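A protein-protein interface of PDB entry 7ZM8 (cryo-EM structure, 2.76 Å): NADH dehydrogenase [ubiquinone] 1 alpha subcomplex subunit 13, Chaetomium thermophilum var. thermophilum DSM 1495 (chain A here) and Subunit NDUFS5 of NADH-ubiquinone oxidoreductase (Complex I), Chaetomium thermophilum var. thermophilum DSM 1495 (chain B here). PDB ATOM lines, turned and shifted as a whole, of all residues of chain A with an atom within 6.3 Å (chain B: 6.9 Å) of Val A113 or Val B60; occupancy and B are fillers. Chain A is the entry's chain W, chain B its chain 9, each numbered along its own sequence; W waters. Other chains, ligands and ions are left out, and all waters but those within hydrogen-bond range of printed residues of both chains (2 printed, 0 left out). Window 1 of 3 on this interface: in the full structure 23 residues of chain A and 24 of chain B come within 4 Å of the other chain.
Water W2 bridges OE1 of Glu B56 (2.6 Å) and O of Phe A111 (2.7 Å).
Water W1 lies within hydrogen-bond range of the side-chain hydroxyl of Thr A114, the side-chain amide oxygen of Gln B64 and the backbone carbonyl oxygen of Ala A112.
NH2 of Arg B59 lies within salt-bridge range of OD2 of Asp A86.
The side-chain carboxylate (OE1) of Glu B56 is in hydrogen-bond range of the backbone NH (N) of Phe A111 (3.0 Å).
The side-chain hydroxyl (OG1) of Thr A114 lies within hydrogen-bond range of the side-chain amide oxygen (OE1) of Gln B64, 3.4 Å away.
OG1 of Thr A114 is in hydrogen-bond range of NH1 of Arg B68, 2.9 Å away.
Among the printed residues, pairs that only touch across the chains: Val A113 with Tyr B67 (3.4 Å), Ala A112 with Val B60 (3.5 Å), Val A113 with Gln B64 (3.6 Å), Pro A115 with Arg B68 (3.6 Å), Val A113 with Leu B63 (3.7 Å), Phe A111 with Ala B57 (3.7 Å), Asp A86 with Leu B63 (3.8 Å) and Val A113 with Val B60 (3.9 Å).
Of the 14 printed residues of chain B, 8 touch a printed residue of chain A.
Of the 7 printed residues of chain A, 6 touch a printed residue of chain B.
Hydrophobic or aromatic side chains of chain A that line the printed part of chain B: Phe A111 and Val A113.
Among the printed residues, Asp or Glu carboxylates within 4 Å of a Lys or Arg side-chain nitrogen of the other chain: Asp A86 with Arg B59 (3.1 Å).
The side-chain amide oxygen (OE1) of Gln B64 sits at hydrogen-bond distance from the guanidinium group (NH1) of Arg B68, 2.8 Å away.
Of chain B, only Val B60, Leu B63, Gln B64 and Tyr B67 come within 4 Å of Val A113.
Printed residues of chain B within 4 Å of Thr A114: Gln B64 and Arg B68.
Printed residues of chain B within 4 Å of Pro A115: Arg B68.
Of the printed residues of chain A, Arg B59 touches Asp A86 (3.1 Å).
Of the printed residues of chain A, Leu B63 touches Asp A86 (3.8 Å) and Val A113 (3.7 Å).
Printed residues of chain A within 4 Å of Arg B68: Thr A114 (2.9 Å) and Pro A115 (3.6 Å).
The nearest printed residue of chain A that does not touch Val B60 is Phe A111 (4.01 Å).
The nearest printed residue of chain B that does not touch Asp A86 is Val B60 (6.1 Å).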
ATOM      1  N   ASP A  86     -17.076 -11.316 -37.278  1.00  0.00           N
ATOM      2  CA  ASP A  86     -16.128 -11.580 -36.170  1.00  0.00           C
ATOM      3  C   ASP A  86     -15.646 -10.255 -35.587  1.00  0.00           C
ATOM      4  O   ASP A  86     -15.412 -10.183 -34.378  1.00  0.00           O
ATOM      5  CB  ASP A  86     -14.992 -12.483 -36.638  1.00  0.00           C
ATOM      6  CG  ASP A  86     -14.218 -13.122 -35.498  1.00  0.00           C
ATOM      7  OD1 ASP A  86     -14.840 -13.414 -34.458  1.00  0.00           O
ATOM      8  OD2 ASP A  86     -12.996 -13.315 -35.657  1.00  0.00           O
ATOM      9  N   ARG A  89     -18.640  -9.144 -33.555  1.00  0.00           N
ATOM     10  CA  ARG A  89     -18.858 -10.030 -32.385  1.00  0.00           C
ATOM     11  C   ARG A  89     -17.885  -9.619 -31.289  1.00  0.00           C
ATOM     12  O   ARG A  89     -18.293  -9.650 -30.130  1.00  0.00           O
ATOM     13  CB  ARG A  89     -18.646 -11.476 -32.834  1.00  0.00           C
ATOM     14  CG  ARG A  89     -19.340 -12.516 -31.971  1.00  0.00           C
ATOM     15  CD  ARG A  89     -19.298 -13.896 -32.593  1.00  0.00           C
ATOM     16  NE  ARG A  89     -20.258 -14.047 -33.676  1.00  0.00           N
ATOM     17  CZ  ARG A  89     -19.944 -14.141 -34.961  1.00  0.00           C
ATOM     18  NH1 ARG A  89     -20.901 -14.284 -35.859  1.00  0.00           N
ATOM     19  NH2 ARG A  89     -18.682 -14.116 -35.345  1.00  0.00           N
ATOM     20  N   PHE A 111      -7.564 -19.865 -36.284  1.00  0.00           N
ATOM     21  CA  PHE A 111      -8.447 -20.353 -35.207  1.00  0.00           C
ATOM     22  C   PHE A 111      -9.751 -19.576 -35.316  1.00  0.00           C
ATOM     23  O   PHE A 111      -9.757 -18.513 -35.926  1.00  0.00           O
ATOM     24  CB  PHE A 111      -7.779 -20.085 -33.867  1.00  0.00           C
ATOM     25  CG  PHE A 111      -6.376 -20.597 -33.703  1.00  0.00           C
ATOM     26  CD1 PHE A 111      -6.142 -21.928 -33.418  1.00  0.00           C
ATOM     27  CD2 PHE A 111      -5.298 -19.733 -33.774  1.00  0.00           C
ATOM     28  CE1 PHE A 111      -4.852 -22.386 -33.228  1.00  0.00           C
ATOM     29  CE2 PHE A 111      -4.008 -20.200 -33.605  1.00  0.00           C
ATOM     30  CZ  PHE A 111      -3.787 -21.526 -33.332  1.00  0.00           C
ATOM     31  N   ALA A 112     -10.828 -20.120 -34.770  1.00  0.00           N
ATOM     32  CA  ALA A 112     -12.138 -19.432 -34.777  1.00  0.00           C
ATOM     33  C   ALA A 112     -12.811 -19.608 -33.424  1.00  0.00           C
ATOM     34  O   ALA A 112     -12.464 -20.558 -32.711  1.00  0.00           O
ATOM     35  CB  ALA A 112     -13.007 -20.039 -35.835  1.00  0.00           C
ATOM     36  N   VAL A 113     -13.750 -18.737 -33.079  1.00  0.00           N
ATOM     37  CA  VAL A 113     -14.516 -18.954 -31.817  1.00  0.00           C
ATOM     38  C   VAL A 113     -15.579 -19.976 -32.169  1.00  0.00           C
ATOM     39  O   VAL A 113     -16.145 -19.882 -33.255  1.00  0.00           O
ATOM     40  CB  VAL A 113     -15.104 -17.662 -31.222  1.00  0.00           C
ATOM     41  CG1 VAL A 113     -16.089 -17.927 -30.106  1.00  0.00           C
ATOM     42  CG2 VAL A 113     -14.017 -16.702 -30.784  1.00  0.00           C
ATOM     43  N   THR A 114     -15.793 -20.944 -31.289  1.00  0.00           N
ATOM     44  CA  THR A 114     -16.728 -22.038 -31.606  1.00  0.00           C
ATOM     45  C   THR A 114     -17.782 -22.106 -30.514  1.00  0.00           C
ATOM     46  O   THR A 114     -17.482 -21.726 -29.378  1.00  0.00           O
ATOM     47  CB  THR A 114     -15.981 -23.367 -31.771  1.00  0.00           C
ATOM     48  OG1 THR A 114     -15.093 -23.515 -30.665  1.00  0.00           O
ATOM     49  CG2 THR A 114     -15.218 -23.471 -33.073  1.00  0.00           C
ATOM     50  N   PRO A 115     -19.041 -22.530 -30.796  1.00  0.00           N
ATOM     51  CA  PRO A 115     -20.003 -22.728 -29.729  1.00  0.00           C
ATOM     52  C   PRO A 115     -19.485 -23.825 -28.796  1.00  0.00           C
ATOM     53  O   PRO A 115     -18.746 -24.672 -29.240  1.00  0.00           O
ATOM     54  CB  PRO A 115     -21.262 -23.208 -30.449  1.00  0.00           C
ATOM     55  CG  PRO A 115     -21.140 -22.620 -31.824  1.00  0.00           C
ATOM     56  CD  PRO A 115     -19.667 -22.765 -32.117  1.00  0.00           C
ATOM     57  N   LYS B  55      -0.217 -14.696 -31.175  1.00  0.00           N
ATOM     58  CA  LYS B  55      -1.069 -13.531 -30.822  1.00  0.00           C
ATOM     59  C   LYS B  55      -2.520 -13.799 -31.226  1.00  0.00           C
ATOM     60  O   LYS B  55      -3.406 -13.362 -30.498  1.00  0.00           O
ATOM     61  CB  LYS B  55      -0.531 -12.237 -31.439  1.00  0.00           C
ATOM     62  CG  LYS B  55       0.954 -11.980 -31.277  1.00  0.00           C
ATOM     63  CD  LYS B  55       1.428 -10.848 -32.146  1.00  0.00           C
ATOM     64  CE  LYS B  55       0.530  -9.636 -32.058  1.00  0.00           C
ATOM     65  NZ  LYS B  55       0.632  -8.958 -30.746  1.00  0.00           N
ATOM     66  N   GLU B  56      -2.750 -14.432 -32.383  1.00  0.00           N
ATOM     67  CA  GLU B  56      -4.111 -14.790 -32.848  1.00  0.00           C
ATOM     68  C   GLU B  56      -4.749 -15.797 -31.905  1.00  0.00           C
ATOM     69  O   GLU B  56      -5.944 -15.674 -31.636  1.00  0.00           O
ATOM     70  CB  GLU B  56      -4.005 -15.441 -34.212  1.00  0.00           C
ATOM     71  CG  GLU B  56      -5.355 -15.696 -34.849  1.00  0.00           C
ATOM     72  CD  GLU B  56      -5.311 -16.471 -36.149  1.00  0.00           C
ATOM     73  OE1 GLU B  56      -6.323 -17.097 -36.484  1.00  0.00           O
ATOM     74  OE2 GLU B  56      -4.273 -16.440 -36.821  1.00  0.00           O
ATOM     75  N   ALA B  57      -3.982 -16.784 -31.464  1.00  0.00           N
ATOM     76  CA  ALA B  57      -4.470 -17.790 -30.506  1.00  0.00           C
ATOM     77  C   ALA B  57      -4.907 -17.078 -29.237  1.00  0.00           C
ATOM     78  O   ALA B  57      -5.941 -17.440 -28.684  1.00  0.00           O
ATOM     79  CB  ALA B  57      -3.338 -18.733 -30.251  1.00  0.00           C
ATOM     80  N   ALA B  58      -4.118 -16.109 -28.799  1.00  0.00           N
ATOM     81  CA  ALA B  58      -4.425 -15.332 -27.583  1.00  0.00           C
ATOM     82  C   ALA B  58      -5.706 -14.519 -27.753  1.00  0.00           C
ATOM     83  O   ALA B  58      -6.512 -14.506 -26.808  1.00  0.00           O
ATOM     84  CB  ALA B  58      -3.264 -14.443 -27.278  1.00  0.00           C
ATOM     85  N   ARG B  59      -5.895 -13.889 -28.909  1.00  0.00           N
ATOM     86  CA  ARG B  59      -7.154 -13.151 -29.158  1.00  0.00           C
ATOM     87  C   ARG B  59      -8.325 -14.123 -29.115  1.00  0.00           C
ATOM     88  O   ARG B  59      -9.318 -13.792 -28.477  1.00  0.00           O
ATOM     89  CB  ARG B  59      -7.130 -12.495 -30.539  1.00  0.00           C
ATOM     90  CG  ARG B  59      -8.446 -11.856 -30.955  1.00  0.00           C
ATOM     91  CD  ARG B  59      -8.375 -11.247 -32.339  1.00  0.00           C
ATOM     92  NE  ARG B  59      -9.679 -10.843 -32.836  1.00  0.00           N
ATOM     93  CZ  ARG B  59     -10.453 -11.596 -33.607  1.00  0.00           C
ATOM     94  NH1 ARG B  59     -10.044 -12.796 -33.978  1.00  0.00           N
ATOM     95  NH2 ARG B  59     -11.627 -11.143 -34.010  1.00  0.00           N
ATOM     96  N   VAL B  60      -8.204 -15.274 -29.769  1.00  0.00           N
ATOM     97  CA  VAL B  60      -9.344 -16.230 -29.851  1.00  0.00           C
ATOM     98  C   VAL B  60      -9.643 -16.831 -28.479  1.00  0.00           C
ATOM     99  O   VAL B  60     -10.806 -16.976 -28.163  1.00  0.00           O
ATOM    100  CB  VAL B  60      -9.220 -17.261 -30.994  1.00  0.00           C
ATOM    101  CG1 VAL B  60     -10.418 -18.194 -31.045  1.00  0.00           C
ATOM    102  CG2 VAL B  60      -9.038 -16.590 -32.346  1.00  0.00           C
ATOM    103  N   ARG B  61      -8.635 -17.143 -27.686  1.00  0.00           N
ATOM    104  CA  ARG B  61      -8.923 -17.818 -26.401  1.00  0.00           C
ATOM    105  C   ARG B  61      -9.769 -16.867 -25.569  1.00  0.00           C
ATOM    106  O   ARG B  61     -10.704 -17.341 -24.914  1.00  0.00           O
ATOM    107  CB  ARG B  61      -7.625 -18.297 -25.743  1.00  0.00           C
ATOM    108  CG  ARG B  61      -7.189 -19.684 -26.190  1.00  0.00           C
ATOM    109  CD  ARG B  61      -5.967 -20.231 -25.478  1.00  0.00           C
ATOM    110  NE  ARG B  61      -4.749 -20.138 -26.270  1.00  0.00           N
ATOM    111  CZ  ARG B  61      -3.850 -19.167 -26.165  1.00  0.00           C
ATOM    112  NH1 ARG B  61      -4.016 -18.195 -25.285  1.00  0.00           N
ATOM    113  NH2 ARG B  61      -2.780 -19.176 -26.934  1.00  0.00           N
ATOM    114  N   ALA B  62      -9.452 -15.576 -25.608  1.00  0.00           N
ATOM    115  CA  ALA B  62     -10.194 -14.536 -24.869  1.00  0.00           C
ATOM    116  C   ALA B  62     -11.584 -14.342 -25.460  1.00  0.00           C
ATOM    117  O   ALA B  62     -12.548 -14.338 -24.708  1.00  0.00           O
ATOM    118  CB  ALA B  62      -9.423 -13.273 -25.042  1.00  0.00           C
ATOM    119  N   LEU B  63     -11.647 -14.100 -26.758  1.00  0.00           N
ATOM    120  CA  LEU B  63     -12.928 -13.853 -27.404  1.00  0.00           C
ATOM    121  C   LEU B  63     -13.844 -15.061 -27.284  1.00  0.00           C
ATOM    122  O   LEU B  63     -15.066 -14.915 -27.162  1.00  0.00           O
ATOM    123  CB  LEU B  63     -12.702 -13.488 -28.869  1.00  0.00           C
ATOM    124  CG  LEU B  63     -13.926 -13.177 -29.728  1.00  0.00           C
ATOM    125  CD1 LEU B  63     -14.888 -12.258 -28.995  1.00  0.00           C
ATOM    126  CD2 LEU B  63     -13.506 -12.573 -31.052  1.00  0.00           C
ATOM    127  N   GLN B  64     -13.272 -16.261 -27.324  1.00  0.00           N
ATOM    128  CA  GLN B  64     -14.056 -17.477 -27.173  1.00  0.00           C
ATOM    129  C   GLN B  64     -14.563 -17.637 -25.750  1.00  0.00           C
ATOM    130  O   GLN B  64     -15.655 -18.171 -25.540  1.00  0.00           O
ATOM    131  CB  GLN B  64     -13.195 -18.667 -27.574  1.00  0.00           C
ATOM    132  CG  GLN B  64     -13.840 -20.014 -27.577  1.00  0.00           C
ATOM    133  CD  GLN B  64     -12.856 -21.041 -28.046  1.00  0.00           C
ATOM    134  OE1 GLN B  64     -13.195 -22.213 -28.162  1.00  0.00           O
ATOM    135  NE2 GLN B  64     -11.636 -20.629 -28.302  1.00  0.00           N
ATOM    136  N   ALA B  65     -13.786 -17.187 -24.766  1.00  0.00           N
ATOM    137  CA  ALA B  65     -14.221 -17.270 -23.378  1.00  0.00           C
ATOM    138  C   ALA B  65     -15.322 -16.262 -23.084  1.00  0.00           C
ATOM    139  O   ALA B  65     -16.205 -16.523 -22.260  1.00  0.00           O
ATOM    140  CB  ALA B  65     -13.032 -17.059 -22.446  1.00  0.00           C
ATOM    141  N   ALA B  66     -15.280 -15.102 -23.735  1.00  0.00           N
ATOM    142  CA  ALA B  66     -16.365 -14.143 -23.588  1.00  0.00           C
ATOM    143  C   ALA B  66     -17.611 -14.598 -24.328  1.00  0.00           C
ATOM    144  O   ALA B  66     -18.730 -14.344 -23.873  1.00  0.00           O
ATOM    145  CB  ALA B  66     -15.928 -12.772 -24.089  1.00  0.00           C
ATOM    146  N   TYR B  67     -17.435 -15.254 -25.472  1.00  0.00           N
ATOM    147  CA  TYR B  67     -18.577 -15.714 -26.253  1.00  0.00           C
ATOM    148  C   TYR B  67     -19.315 -16.827 -25.530  1.00  0.00           C
ATOM    149  O   TYR B  67     -20.548 -16.830 -25.466  1.00  0.00           O
ATOM    150  CB  TYR B  67     -18.098 -16.178 -27.627  1.00  0.00           C
ATOM    151  CG  TYR B  67     -19.165 -16.801 -28.490  1.00  0.00           C
ATOM    152  CD1 TYR B  67     -20.111 -16.018 -29.126  1.00  0.00           C
ATOM    153  CD2 TYR B  67     -19.215 -18.170 -28.682  1.00  0.00           C
ATOM    154  CE1 TYR B  67     -21.078 -16.580 -29.914  1.00  0.00           C
ATOM    155  CE2 TYR B  67     -20.181 -18.740 -29.467  1.00  0.00           C
ATOM    156  CZ  TYR B  67     -21.109 -17.941 -30.079  1.00  0.00           C
ATOM    157  OH  TYR B  67     -22.077 -18.511 -30.871  1.00  0.00           O
ATOM    158  N   ARG B  68     -18.576 -17.784 -24.980  1.00  0.00           N
ATOM    159  CA  ARG B  68     -19.212 -18.888 -24.280  1.00  0.00           C
ATOM    160  C   ARG B  68     -19.864 -18.439 -22.981  1.00  0.00           C
ATOM    161  O   ARG B  68     -20.939 -18.935 -22.633  1.00  0.00           O
ATOM    162  CB  ARG B  68     -18.198 -20.002 -24.037  1.00  0.00           C
ATOM    163  CG  ARG B  68     -18.204 -21.050 -25.132  1.00  0.00           C
ATOM    164  CD  ARG B  68     -17.027 -21.992 -25.042  1.00  0.00           C
ATOM    165  NE  ARG B  68     -16.574 -22.412 -26.360  1.00  0.00           N
ATOM    166  CZ  ARG B  68     -15.846 -23.498 -26.578  1.00  0.00           C
ATOM    167  NH1 ARG B  68     -15.498 -23.834 -27.807  1.00  0.00           N
ATOM    168  NH2 ARG B  68     -15.468 -24.256 -25.563  1.00  0.00           N
HETATM  169  O   HOH W   1     -12.426 -22.766 -30.829  1.00  0.00           O
HETATM  170  O   HOH W   2      -8.668 -16.084 -36.478  1.00  0.00           O
